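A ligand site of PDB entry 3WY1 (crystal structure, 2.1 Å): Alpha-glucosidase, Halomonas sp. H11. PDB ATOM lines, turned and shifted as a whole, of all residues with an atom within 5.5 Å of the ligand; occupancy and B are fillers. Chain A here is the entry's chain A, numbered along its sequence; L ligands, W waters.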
ATOM      1  N   ASP A  62     -27.381 -21.576  13.327  1.00  0.00           N
ATOM      2  CA  ASP A  62     -27.015 -20.677  12.227  1.00  0.00           C
ATOM      3  C   ASP A  62     -26.669 -19.332  12.847  1.00  0.00           C
ATOM      4  O   ASP A  62     -27.012 -18.257  12.320  1.00  0.00           O
ATOM      5  CB  ASP A  62     -28.148 -20.584  11.209  1.00  0.00           C
ATOM      6  CG  ASP A  62     -27.760 -19.799   9.954  1.00  0.00           C
ATOM      7  OD1 ASP A  62     -26.549 -19.557   9.702  1.00  0.00           O
ATOM      8  OD2 ASP A  62     -28.697 -19.436   9.204  1.00  0.00           O
ATOM      9  N   TYR A  65     -29.499 -16.737  13.428  1.00  0.00           N
ATOM     10  CA  TYR A  65     -30.553 -16.737  12.426  1.00  0.00           C
ATOM     11  C   TYR A  65     -31.561 -17.883  12.606  1.00  0.00           C
ATOM     12  O   TYR A  65     -32.520 -18.001  11.833  1.00  0.00           O
ATOM     13  CB  TYR A  65     -29.969 -16.695  11.015  1.00  0.00           C
ATOM     14  CG  TYR A  65     -29.413 -15.328  10.688  1.00  0.00           C
ATOM     15  CD1 TYR A  65     -30.245 -14.287  10.269  1.00  0.00           C
ATOM     16  CD2 TYR A  65     -28.050 -15.058  10.821  1.00  0.00           C
ATOM     17  CE1 TYR A  65     -29.738 -13.020   9.989  1.00  0.00           C
ATOM     18  CE2 TYR A  65     -27.541 -13.807  10.533  1.00  0.00           C
ATOM     19  CZ  TYR A  65     -28.381 -12.782  10.120  1.00  0.00           C
ATOM     20  OH  TYR A  65     -27.855 -11.530   9.858  1.00  0.00           O
ATOM     21  N   VAL A 102     -35.871 -11.898  11.735  1.00  0.00           N
ATOM     22  CA  VAL A 102     -35.771 -13.131  10.972  1.00  0.00           C
ATOM     23  C   VAL A 102     -37.105 -13.864  11.031  1.00  0.00           C
ATOM     24  O   VAL A 102     -37.278 -14.759  11.856  1.00  0.00           O
ATOM     25  CB  VAL A 102     -34.638 -14.018  11.520  1.00  0.00           C
ATOM     26  CG1 VAL A 102     -34.281 -15.131  10.533  1.00  0.00           C
ATOM     27  CG2 VAL A 102     -33.421 -13.154  11.792  1.00  0.00           C
ATOM     28  N   HIS A 105     -38.414 -17.856   8.915  1.00  0.00           N
ATOM     29  CA  HIS A 105     -38.283 -19.174   9.548  1.00  0.00           C
ATOM     30  C   HIS A 105     -37.925 -18.998  11.013  1.00  0.00           C
ATOM     31  O   HIS A 105     -37.381 -17.963  11.409  1.00  0.00           O
ATOM     32  CB  HIS A 105     -37.191 -19.985   8.855  1.00  0.00           C
ATOM     33  CG  HIS A 105     -35.937 -19.216   8.589  1.00  0.00           C
ATOM     34  ND1 HIS A 105     -35.637 -18.673   7.358  1.00  0.00           N
ATOM     35  CD2 HIS A 105     -34.920 -18.852   9.411  1.00  0.00           C
ATOM     36  CE1 HIS A 105     -34.492 -18.025   7.419  1.00  0.00           C
ATOM     37  NE2 HIS A 105     -34.027 -18.115   8.657  1.00  0.00           N
ATOM     38  N   ILE A 146     -30.485 -24.293   0.674  1.00  0.00           N
ATOM     39  CA  ILE A 146     -29.267 -23.554   0.372  1.00  0.00           C
ATOM     40  C   ILE A 146     -28.072 -24.145   1.140  1.00  0.00           C
ATOM     41  O   ILE A 146     -26.929 -24.111   0.675  1.00  0.00           O
ATOM     42  CB  ILE A 146     -29.452 -22.067   0.683  1.00  0.00           C
ATOM     43  CG1 ILE A 146     -30.588 -21.510  -0.161  1.00  0.00           C
ATOM     44  CG2 ILE A 146     -28.160 -21.306   0.450  1.00  0.00           C
ATOM     45  CD1 ILE A 146     -30.903 -20.064   0.082  1.00  0.00           C
ATOM     46  N   PHE A 147     -28.354 -24.681   2.322  1.00  0.00           N
ATOM     47  CA  PHE A 147     -27.302 -25.226   3.179  1.00  0.00           C
ATOM     48  C   PHE A 147     -27.056 -26.721   2.968  1.00  0.00           C
ATOM     49  O   PHE A 147     -26.351 -27.355   3.750  1.00  0.00           O
ATOM     50  CB  PHE A 147     -27.634 -24.928   4.645  1.00  0.00           C
ATOM     51  CG  PHE A 147     -27.540 -23.459   4.999  1.00  0.00           C
ATOM     52  CD1 PHE A 147     -26.869 -22.576   4.179  1.00  0.00           C
ATOM     53  CD2 PHE A 147     -28.126 -22.974   6.176  1.00  0.00           C
ATOM     54  CE1 PHE A 147     -26.772 -21.214   4.501  1.00  0.00           C
ATOM     55  CE2 PHE A 147     -28.030 -21.618   6.510  1.00  0.00           C
ATOM     56  CZ  PHE A 147     -27.361 -20.731   5.668  1.00  0.00           C
ATOM     57  N   PHE A 166     -33.241 -23.176   4.578  1.00  0.00           N
ATOM     58  CA  PHE A 166     -31.947 -23.181   5.217  1.00  0.00           C
ATOM     59  C   PHE A 166     -31.713 -24.457   6.012  1.00  0.00           C
ATOM     60  O   PHE A 166     -31.949 -25.541   5.485  1.00  0.00           O
ATOM     61  CB  PHE A 166     -31.752 -21.885   5.981  1.00  0.00           C
ATOM     62  CG  PHE A 166     -31.804 -20.681   5.078  1.00  0.00           C
ATOM     63  CD1 PHE A 166     -30.688 -20.280   4.354  1.00  0.00           C
ATOM     64  CD2 PHE A 166     -32.985 -19.965   4.900  1.00  0.00           C
ATOM     65  CE1 PHE A 166     -30.738 -19.191   3.496  1.00  0.00           C
ATOM     66  CE2 PHE A 166     -33.040 -18.869   4.053  1.00  0.00           C
ATOM     67  CZ  PHE A 166     -31.918 -18.486   3.352  1.00  0.00           C
ATOM     68  N   GLN A 170     -34.148 -24.863  10.863  1.00  0.00           N
ATOM     69  CA  GLN A 170     -34.784 -23.567  10.575  1.00  0.00           C
ATOM     70  C   GLN A 170     -36.039 -23.786   9.725  1.00  0.00           C
ATOM     71  O   GLN A 170     -36.072 -23.395   8.555  1.00  0.00           O
ATOM     72  CB  GLN A 170     -33.818 -22.642   9.824  1.00  0.00           C
ATOM     73  CG  GLN A 170     -32.716 -21.994  10.668  1.00  0.00           C
ATOM     74  CD  GLN A 170     -31.569 -21.454   9.820  1.00  0.00           C
ATOM     75  OE1 GLN A 170     -30.943 -22.197   9.058  1.00  0.00           O
ATOM     76  NE2 GLN A 170     -31.306 -20.136   9.928  1.00  0.00           N
ATOM     77  N   ARG A 200     -33.358  -4.686   9.511  1.00  0.00           N
ATOM     78  CA  ARG A 200     -32.874  -5.391   8.336  1.00  0.00           C
ATOM     79  C   ARG A 200     -33.697  -6.676   8.261  1.00  0.00           C
ATOM     80  O   ARG A 200     -33.757  -7.462   9.220  1.00  0.00           O
ATOM     81  CB  ARG A 200     -31.373  -5.663   8.429  1.00  0.00           C
ATOM     82  CG  ARG A 200     -30.799  -6.386   7.230  1.00  0.00           C
ATOM     83  CD  ARG A 200     -30.836  -7.879   7.471  1.00  0.00           C
ATOM     84  NE  ARG A 200     -29.990  -8.635   6.556  1.00  0.00           N
ATOM     85  CZ  ARG A 200     -29.811  -9.942   6.638  1.00  0.00           C
ATOM     86  NH1 ARG A 200     -30.424 -10.629   7.592  1.00  0.00           N
ATOM     87  NH2 ARG A 200     -29.023 -10.570   5.768  1.00  0.00           N
ATOM     88  N   ASP A 202     -34.184 -10.129   7.014  1.00  0.00           N
ATOM     89  CA  ASP A 202     -33.554 -11.350   6.529  1.00  0.00           C
ATOM     90  C   ASP A 202     -34.378 -12.073   5.474  1.00  0.00           C
ATOM     91  O   ASP A 202     -35.589 -12.253   5.670  1.00  0.00           O
ATOM     92  CB  ASP A 202     -33.338 -12.285   7.720  1.00  0.00           C
ATOM     93  CG  ASP A 202     -32.572 -13.533   7.347  1.00  0.00           C
ATOM     94  OD1 ASP A 202     -31.351 -13.421   7.108  1.00  0.00           O
ATOM     95  OD2 ASP A 202     -33.192 -14.610   7.283  1.00  0.00           O
ATOM     96  N   THR A 203     -33.738 -12.495   4.385  1.00  0.00           N
ATOM     97  CA  THR A 203     -34.396 -13.269   3.319  1.00  0.00           C
ATOM     98  C   THR A 203     -35.803 -12.758   3.009  1.00  0.00           C
ATOM     99  O   THR A 203     -36.779 -13.514   3.045  1.00  0.00           O
ATOM    100  CB  THR A 203     -34.453 -14.773   3.665  1.00  0.00           C
ATOM    101  OG1 THR A 203     -34.944 -14.934   5.007  1.00  0.00           O
ATOM    102  CG2 THR A 203     -33.085 -15.355   3.628  1.00  0.00           C
ATOM    103  N   PHE A 206     -38.221 -14.515   0.692  1.00  0.00           N
ATOM    104  CA  PHE A 206     -38.479 -15.939   0.915  1.00  0.00           C
ATOM    105  C   PHE A 206     -39.819 -16.175   1.622  1.00  0.00           C
ATOM    106  O   PHE A 206     -40.286 -17.300   1.637  1.00  0.00           O
ATOM    107  CB  PHE A 206     -37.370 -16.580   1.752  1.00  0.00           C
ATOM    108  CG  PHE A 206     -36.074 -16.801   1.023  1.00  0.00           C
ATOM    109  CD1 PHE A 206     -35.502 -18.070   0.972  1.00  0.00           C
ATOM    110  CD2 PHE A 206     -35.409 -15.740   0.425  1.00  0.00           C
ATOM    111  CE1 PHE A 206     -34.295 -18.283   0.302  1.00  0.00           C
ATOM    112  CE2 PHE A 206     -34.189 -15.949  -0.250  1.00  0.00           C
ATOM    113  CZ  PHE A 206     -33.646 -17.228  -0.300  1.00  0.00           C
ATOM    114  N   THR A 226     -27.173 -17.877  -9.966  1.00  0.00           N
ATOM    115  CA  THR A 226     -27.567 -16.826  -9.040  1.00  0.00           C
ATOM    116  C   THR A 226     -26.348 -16.264  -8.302  1.00  0.00           C
ATOM    117  O   THR A 226     -25.364 -16.987  -8.092  1.00  0.00           O
ATOM    118  CB  THR A 226     -28.601 -17.312  -8.015  1.00  0.00           C
ATOM    119  OG1 THR A 226     -28.906 -16.242  -7.111  1.00  0.00           O
ATOM    120  CG2 THR A 226     -28.052 -18.509  -7.218  1.00  0.00           C
ATOM    121  N   GLY A 228     -26.368 -15.147  -5.285  1.00  0.00           N
ATOM    122  CA  GLY A 228     -26.520 -15.394  -3.872  1.00  0.00           C
ATOM    123  C   GLY A 228     -25.960 -16.710  -3.322  1.00  0.00           C
ATOM    124  O   GLY A 228     -26.157 -17.016  -2.139  1.00  0.00           O
ATOM    125  N   ALA A 229     -25.270 -17.478  -4.164  1.00  0.00           N
ATOM    126  CA  ALA A 229     -24.706 -18.778  -3.757  1.00  0.00           C
ATOM    127  C   ALA A 229     -23.474 -19.162  -4.571  1.00  0.00           C
ATOM    128  O   ALA A 229     -23.364 -18.823  -5.754  1.00  0.00           O
ATOM    129  CB  ALA A 229     -25.772 -19.872  -3.837  1.00  0.00           C
ATOM    130  N   TYR A 235     -27.811 -26.015  -5.304  1.00  0.00           N
ATOM    131  CA  TYR A 235     -28.905 -25.040  -5.264  1.00  0.00           C
ATOM    132  C   TYR A 235     -28.887 -24.163  -6.517  1.00  0.00           C
ATOM    133  O   TYR A 235     -29.930 -23.701  -6.975  1.00  0.00           O
ATOM    134  CB  TYR A 235     -28.783 -24.185  -4.002  1.00  0.00           C
ATOM    135  CG  TYR A 235     -29.862 -23.120  -3.792  1.00  0.00           C
ATOM    136  CD1 TYR A 235     -31.092 -23.441  -3.230  1.00  0.00           C
ATOM    137  CD2 TYR A 235     -29.618 -21.786  -4.120  1.00  0.00           C
ATOM    138  CE1 TYR A 235     -32.070 -22.464  -3.023  1.00  0.00           C
ATOM    139  CE2 TYR A 235     -30.583 -20.805  -3.918  1.00  0.00           C
ATOM    140  CZ  TYR A 235     -31.799 -21.137  -3.369  1.00  0.00           C
ATOM    141  OH  TYR A 235     -32.742 -20.136  -3.178  1.00  0.00           O
ATOM    142  N   GLU A 271     -33.236  -7.930   2.685  1.00  0.00           N
ATOM    143  CA  GLU A 271     -32.211  -8.717   1.998  1.00  0.00           C
ATOM    144  C   GLU A 271     -32.845  -9.457   0.832  1.00  0.00           C
ATOM    145  O   GLU A 271     -33.759 -10.253   1.006  1.00  0.00           O
ATOM    146  CB  GLU A 271     -31.573  -9.718   2.972  1.00  0.00           C
ATOM    147  CG  GLU A 271     -30.373 -10.412   2.360  1.00  0.00           C
ATOM    148  CD  GLU A 271     -30.168 -11.813   2.901  1.00  0.00           C
ATOM    149  OE1 GLU A 271     -31.004 -12.287   3.711  1.00  0.00           O
ATOM    150  OE2 GLU A 271     -29.159 -12.442   2.496  1.00  0.00           O
ATOM    151  N   ILE A 272     -32.348  -9.191  -0.374  1.00  0.00           N
ATOM    152  CA  ILE A 272     -32.888  -9.865  -1.551  1.00  0.00           C
ATOM    153  C   ILE A 272     -32.007 -11.037  -1.975  1.00  0.00           C
ATOM    154  O   ILE A 272     -30.797 -10.885  -2.154  1.00  0.00           O
ATOM    155  CB  ILE A 272     -32.994  -8.869  -2.714  1.00  0.00           C
ATOM    156  CG1 ILE A 272     -33.902  -7.689  -2.336  1.00  0.00           C
ATOM    157  CG2 ILE A 272     -33.482  -9.565  -3.978  1.00  0.00           C
ATOM    158  CD1 ILE A 272     -35.402  -8.049  -2.129  1.00  0.00           C
ATOM    159  N   GLY A 273     -32.598 -12.218  -2.124  1.00  0.00           N
ATOM    160  CA  GLY A 273     -31.897 -13.377  -2.666  1.00  0.00           C
ATOM    161  C   GLY A 273     -32.760 -14.022  -3.725  1.00  0.00           C
ATOM    162  O   GLY A 273     -33.644 -14.817  -3.411  1.00  0.00           O
ATOM    163  N   ASP A 274     -32.480 -13.689  -4.982  1.00  0.00           N
ATOM    164  CA  ASP A 274     -33.413 -13.952  -6.086  1.00  0.00           C
ATOM    165  C   ASP A 274     -32.612 -14.126  -7.373  1.00  0.00           C
ATOM    166  O   ASP A 274     -31.488 -13.627  -7.457  1.00  0.00           O
ATOM    167  CB  ASP A 274     -34.344 -12.734  -6.221  1.00  0.00           C
ATOM    168  CG  ASP A 274     -35.464 -12.955  -7.210  1.00  0.00           C
ATOM    169  OD1 ASP A 274     -36.573 -13.362  -6.787  1.00  0.00           O
ATOM    170  OD2 ASP A 274     -35.252 -12.697  -8.410  1.00  0.00           O
ATOM    171  N   TYR A 295     -31.089  -4.411  -0.305  1.00  0.00           N
ATOM    172  CA  TYR A 295     -29.794  -4.639  -0.957  1.00  0.00           C
ATOM    173  C   TYR A 295     -29.765  -5.977  -1.655  1.00  0.00           C
ATOM    174  O   TYR A 295     -30.505  -6.906  -1.285  1.00  0.00           O
ATOM    175  CB  TYR A 295     -28.639  -4.503   0.039  1.00  0.00           C
ATOM    176  CG  TYR A 295     -28.446  -5.657   0.982  1.00  0.00           C
ATOM    177  CD1 TYR A 295     -27.735  -6.790   0.593  1.00  0.00           C
ATOM    178  CD2 TYR A 295     -28.960  -5.615   2.269  1.00  0.00           C
ATOM    179  CE1 TYR A 295     -27.547  -7.865   1.457  1.00  0.00           C
ATOM    180  CE2 TYR A 295     -28.774  -6.695   3.146  1.00  0.00           C
ATOM    181  CZ  TYR A 295     -28.061  -7.800   2.740  1.00  0.00           C
ATOM    182  OH  TYR A 295     -27.869  -8.866   3.602  1.00  0.00           O
ATOM    183  N   PHE A 297     -27.098  -8.904  -4.030  1.00  0.00           N
ATOM    184  CA  PHE A 297     -25.747  -9.469  -4.075  1.00  0.00           C
ATOM    185  C   PHE A 297     -24.983  -9.032  -5.315  1.00  0.00           C
ATOM    186  O   PHE A 297     -23.908  -9.568  -5.599  1.00  0.00           O
ATOM    187  CB  PHE A 297     -25.812 -10.986  -3.970  1.00  0.00           C
ATOM    188  CG  PHE A 297     -25.884 -11.482  -2.553  1.00  0.00           C
ATOM    189  CD1 PHE A 297     -24.823 -12.174  -1.989  1.00  0.00           C
ATOM    190  CD2 PHE A 297     -27.005 -11.238  -1.777  1.00  0.00           C
ATOM    191  CE1 PHE A 297     -24.872 -12.614  -0.676  1.00  0.00           C
ATOM    192  CE2 PHE A 297     -27.071 -11.669  -0.461  1.00  0.00           C
ATOM    193  CZ  PHE A 297     -25.999 -12.374   0.081  1.00  0.00           C
ATOM    194  N   HIS A 332     -21.880 -10.206   6.562  1.00  0.00           N
ATOM    195  CA  HIS A 332     -21.529 -11.410   7.327  1.00  0.00           C
ATOM    196  C   HIS A 332     -21.661 -12.706   6.522  1.00  0.00           C
ATOM    197  O   HIS A 332     -21.433 -13.795   7.046  1.00  0.00           O
ATOM    198  CB  HIS A 332     -22.381 -11.473   8.571  1.00  0.00           C
ATOM    199  CG  HIS A 332     -23.839 -11.648   8.278  1.00  0.00           C
ATOM    200  ND1 HIS A 332     -24.570 -10.674   7.617  1.00  0.00           N
ATOM    201  CD2 HIS A 332     -24.680 -12.668   8.518  1.00  0.00           C
ATOM    202  CE1 HIS A 332     -25.814 -11.100   7.478  1.00  0.00           C
ATOM    203  NE2 HIS A 332     -25.917 -12.302   8.012  1.00  0.00           N
ATOM    204  N   ASP A 333     -22.058 -12.590   5.256  1.00  0.00           N
ATOM    205  CA  ASP A 333     -22.305 -13.747   4.416  1.00  0.00           C
ATOM    206  C   ASP A 333     -21.305 -13.895   3.285  1.00  0.00           C
ATOM    207  O   ASP A 333     -21.359 -14.875   2.551  1.00  0.00           O
ATOM    208  CB  ASP A 333     -23.710 -13.667   3.830  1.00  0.00           C
ATOM    209  CG  ASP A 333     -24.806 -13.880   4.872  1.00  0.00           C
ATOM    210  OD1 ASP A 333     -24.650 -14.754   5.760  1.00  0.00           O
ATOM    211  OD2 ASP A 333     -25.818 -13.142   4.829  1.00  0.00           O
ATOM    212  N   TYR A 389     -22.534 -23.962   7.192  1.00  0.00           N
ATOM    213  CA  TYR A 389     -22.424 -23.761   5.759  1.00  0.00           C
ATOM    214  C   TYR A 389     -20.975 -23.950   5.296  1.00  0.00           C
ATOM    215  O   TYR A 389     -20.692 -23.992   4.082  1.00  0.00           O
ATOM    216  CB  TYR A 389     -22.918 -22.353   5.393  1.00  0.00           C
ATOM    217  CG  TYR A 389     -23.289 -22.145   3.929  1.00  0.00           C
ATOM    218  CD1 TYR A 389     -23.389 -23.215   3.047  1.00  0.00           C
ATOM    219  CD2 TYR A 389     -23.564 -20.865   3.446  1.00  0.00           C
ATOM    220  CE1 TYR A 389     -23.743 -23.017   1.708  1.00  0.00           C
ATOM    221  CE2 TYR A 389     -23.926 -20.663   2.109  1.00  0.00           C
ATOM    222  CZ  TYR A 389     -24.013 -21.741   1.255  1.00  0.00           C
ATOM    223  OH  TYR A 389     -24.369 -21.535  -0.063  1.00  0.00           O
ATOM    224  N   ARG A 400     -18.645 -19.149   5.801  1.00  0.00           N
ATOM    225  CA  ARG A 400     -18.638 -17.717   5.998  1.00  0.00           C
ATOM    226  C   ARG A 400     -17.790 -17.242   7.182  1.00  0.00           C
ATOM    227  O   ARG A 400     -17.747 -16.043   7.469  1.00  0.00           O
ATOM    228  CB  ARG A 400     -20.092 -17.225   6.155  1.00  0.00           C
ATOM    229  CG  ARG A 400     -20.926 -17.427   4.901  1.00  0.00           C
ATOM    230  CD  ARG A 400     -22.438 -17.350   5.193  1.00  0.00           C
ATOM    231  NE  ARG A 400     -22.901 -18.470   6.038  1.00  0.00           N
ATOM    232  CZ  ARG A 400     -24.144 -18.574   6.496  1.00  0.00           C
ATOM    233  NH1 ARG A 400     -25.041 -17.645   6.195  1.00  0.00           N
ATOM    234  NH2 ARG A 400     -24.484 -19.618   7.266  1.00  0.00           N
HETATM  235  O1  LIG L   1     -28.196 -14.871  -1.054  1.00  0.00           O
HETATM  236  O2  LIG L   1     -29.519 -16.322  -1.985  1.00  0.00           O
HETATM  237  C1  LIG L   1     -28.819 -15.958  -0.988  1.00  0.00           C
HETATM  238  C2  LIG L   1     -28.706 -16.808   0.261  1.00  0.00           C
HETATM  239  C3  LIG L   1     -29.591 -16.340   1.397  1.00  0.00           C
HETATM  240  C4  LIG L   1     -27.421 -16.126   2.686  1.00  0.00           C
HETATM  241  O3  LIG L   1     -26.629 -17.113   2.454  1.00  0.00           O
HETATM  242  O4  LIG L   1     -26.893 -15.000   2.855  1.00  0.00           O
HETATM  243  C5  LIG L   1     -29.613 -15.059   3.408  1.00  0.00           C
HETATM  244  C6  LIG L   1     -28.444 -14.316   5.483  1.00  0.00           C
HETATM  245  O5  LIG L   1     -28.353 -13.130   5.928  1.00  0.00           O
HETATM  246  O6  LIG L   1     -27.413 -15.080   5.515  1.00  0.00           O
HETATM  247  C7  LIG L   1     -31.014 -17.067   7.671  1.00  0.00           C
HETATM  248  C8  LIG L   1     -29.823 -16.374   7.013  1.00  0.00           C
HETATM  249  C9  LIG L   1     -30.243 -16.102   5.594  1.00  0.00           C
HETATM  250  C10 LIG L   1     -28.610 -17.285   6.857  1.00  0.00           C
HETATM  251  O7  LIG L   1     -28.412 -17.815   5.738  1.00  0.00           O
HETATM  252  O8  LIG L   1     -27.763 -17.517   7.780  1.00  0.00           O
HETATM  253  C11 LIG L   1     -29.750 -14.843   4.914  1.00  0.00           C
HETATM  254  C12 LIG L   1     -28.933 -16.264   2.776  1.00  0.00           C
HETATM  255  O   HOH W   1     -25.449 -18.959  -0.161  1.00  0.00           O
HETATM  256  O   HOH W   2     -26.504 -15.231   7.748  1.00  0.00           O
HETATM  257  O   HOH W   3     -25.542 -16.994   9.663  1.00  0.00           O
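O8 of the ligand sits close to OD2 of Asp 62, at 2.6 Å.
O6 of the ligand lies close to OD2 of Asp 333, at 2.6 Å.
NH2 of Arg 200 lies within salt-bridge range of O5 of the ligand, at 2.7 Å.
O8 of the ligand is in salt-bridge range of NH1 of Arg 400.
O5 of the ligand is in hydrogen-bond range of NE2 of His 332 (3.3 Å).
The guanidinium group of Arg 400 is in salt-bridge range of the side-chain carboxylate of Asp 62.
NE2 of Gln 170 lies within hydrogen-bond range of OD2 of Asp 62, at 2.8 Å.
The guanidinium group (NH2) of Arg 200 is in salt-bridge range of the side-chain carboxylate (OE1) of Glu 271 (3.3 Å).
NH1 of Arg 200 is in salt-bridge range of OD1 of Asp 202, at 3.0 Å.
The guanidinium group (NH2) of Arg 200 sits at hydrogen-bond distance from the side-chain hydroxyl (OH) of Tyr 295 (3.0 Å).
OD2 of Asp 202 lies within hydrogen-bond range of OG1 of Thr 203.
N of Gly 228 lies close to OG1 of Thr 226.
The backbone carbonyl oxygen (O) of Tyr 65 lies within hydrogen-bond range of the side-chain amide nitrogen (NE2) of Gln 170 (3.1 Å).
The side-chain carboxylate (OD1) of Asp 202 lies close to an oxygen (O5) of the ligand, at 3.2 Å.
The backbone carbonyl oxygen of Gly 228 lies close to an oxygen (O1) of the ligand, 3.2 Å away.
O4 of the ligand lies close to OE2 of Glu 271 (3.4 Å).
Tyr 65 touches the ligand.
NE2 of His 105 touches C7 of the ligand (3.3 Å).
Ile 146 touches the ligand (CD1 to C2, 3.9 Å).
CZ of Phe 147 touches O7 of the ligand, 3.1 Å away.
CE1 of Phe 166 touches O7 of the ligand (3.5 Å).
NE2 of Gln 170 touches C7 of the ligand, at 3.8 Å.
Thr 203 touches the ligand.
CA of Gly 273 touches O2 of the ligand, 3.8 Å away.
CE2 of Phe 297 touches O1 of the ligand (3.4 Å).
Hydrophobic or aromatic side chains within 4 Å of the ligand: Tyr 65, His 105, Ile 146, Phe 147, Phe 166, Phe 297 and His 332.
Of the 26 residues printed, 17 come within 4 Å of the ligand.
Water W2 lies within hydrogen-bond range of O6 of the ligand, OD1 of Asp 333, NE2 of His 332 and NH1 of Arg 400.
Water W3 lies within hydrogen-bond range of the side-chain carboxylate (OD1) of Asp 62 and an oxygen (O8) of the ligand.
Water W1 lies within hydrogen-bond range of OH of Tyr 389 (2.8 Å), O of Gly 228 (2.9 Å) and O3 of the ligand (3.4 Å).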
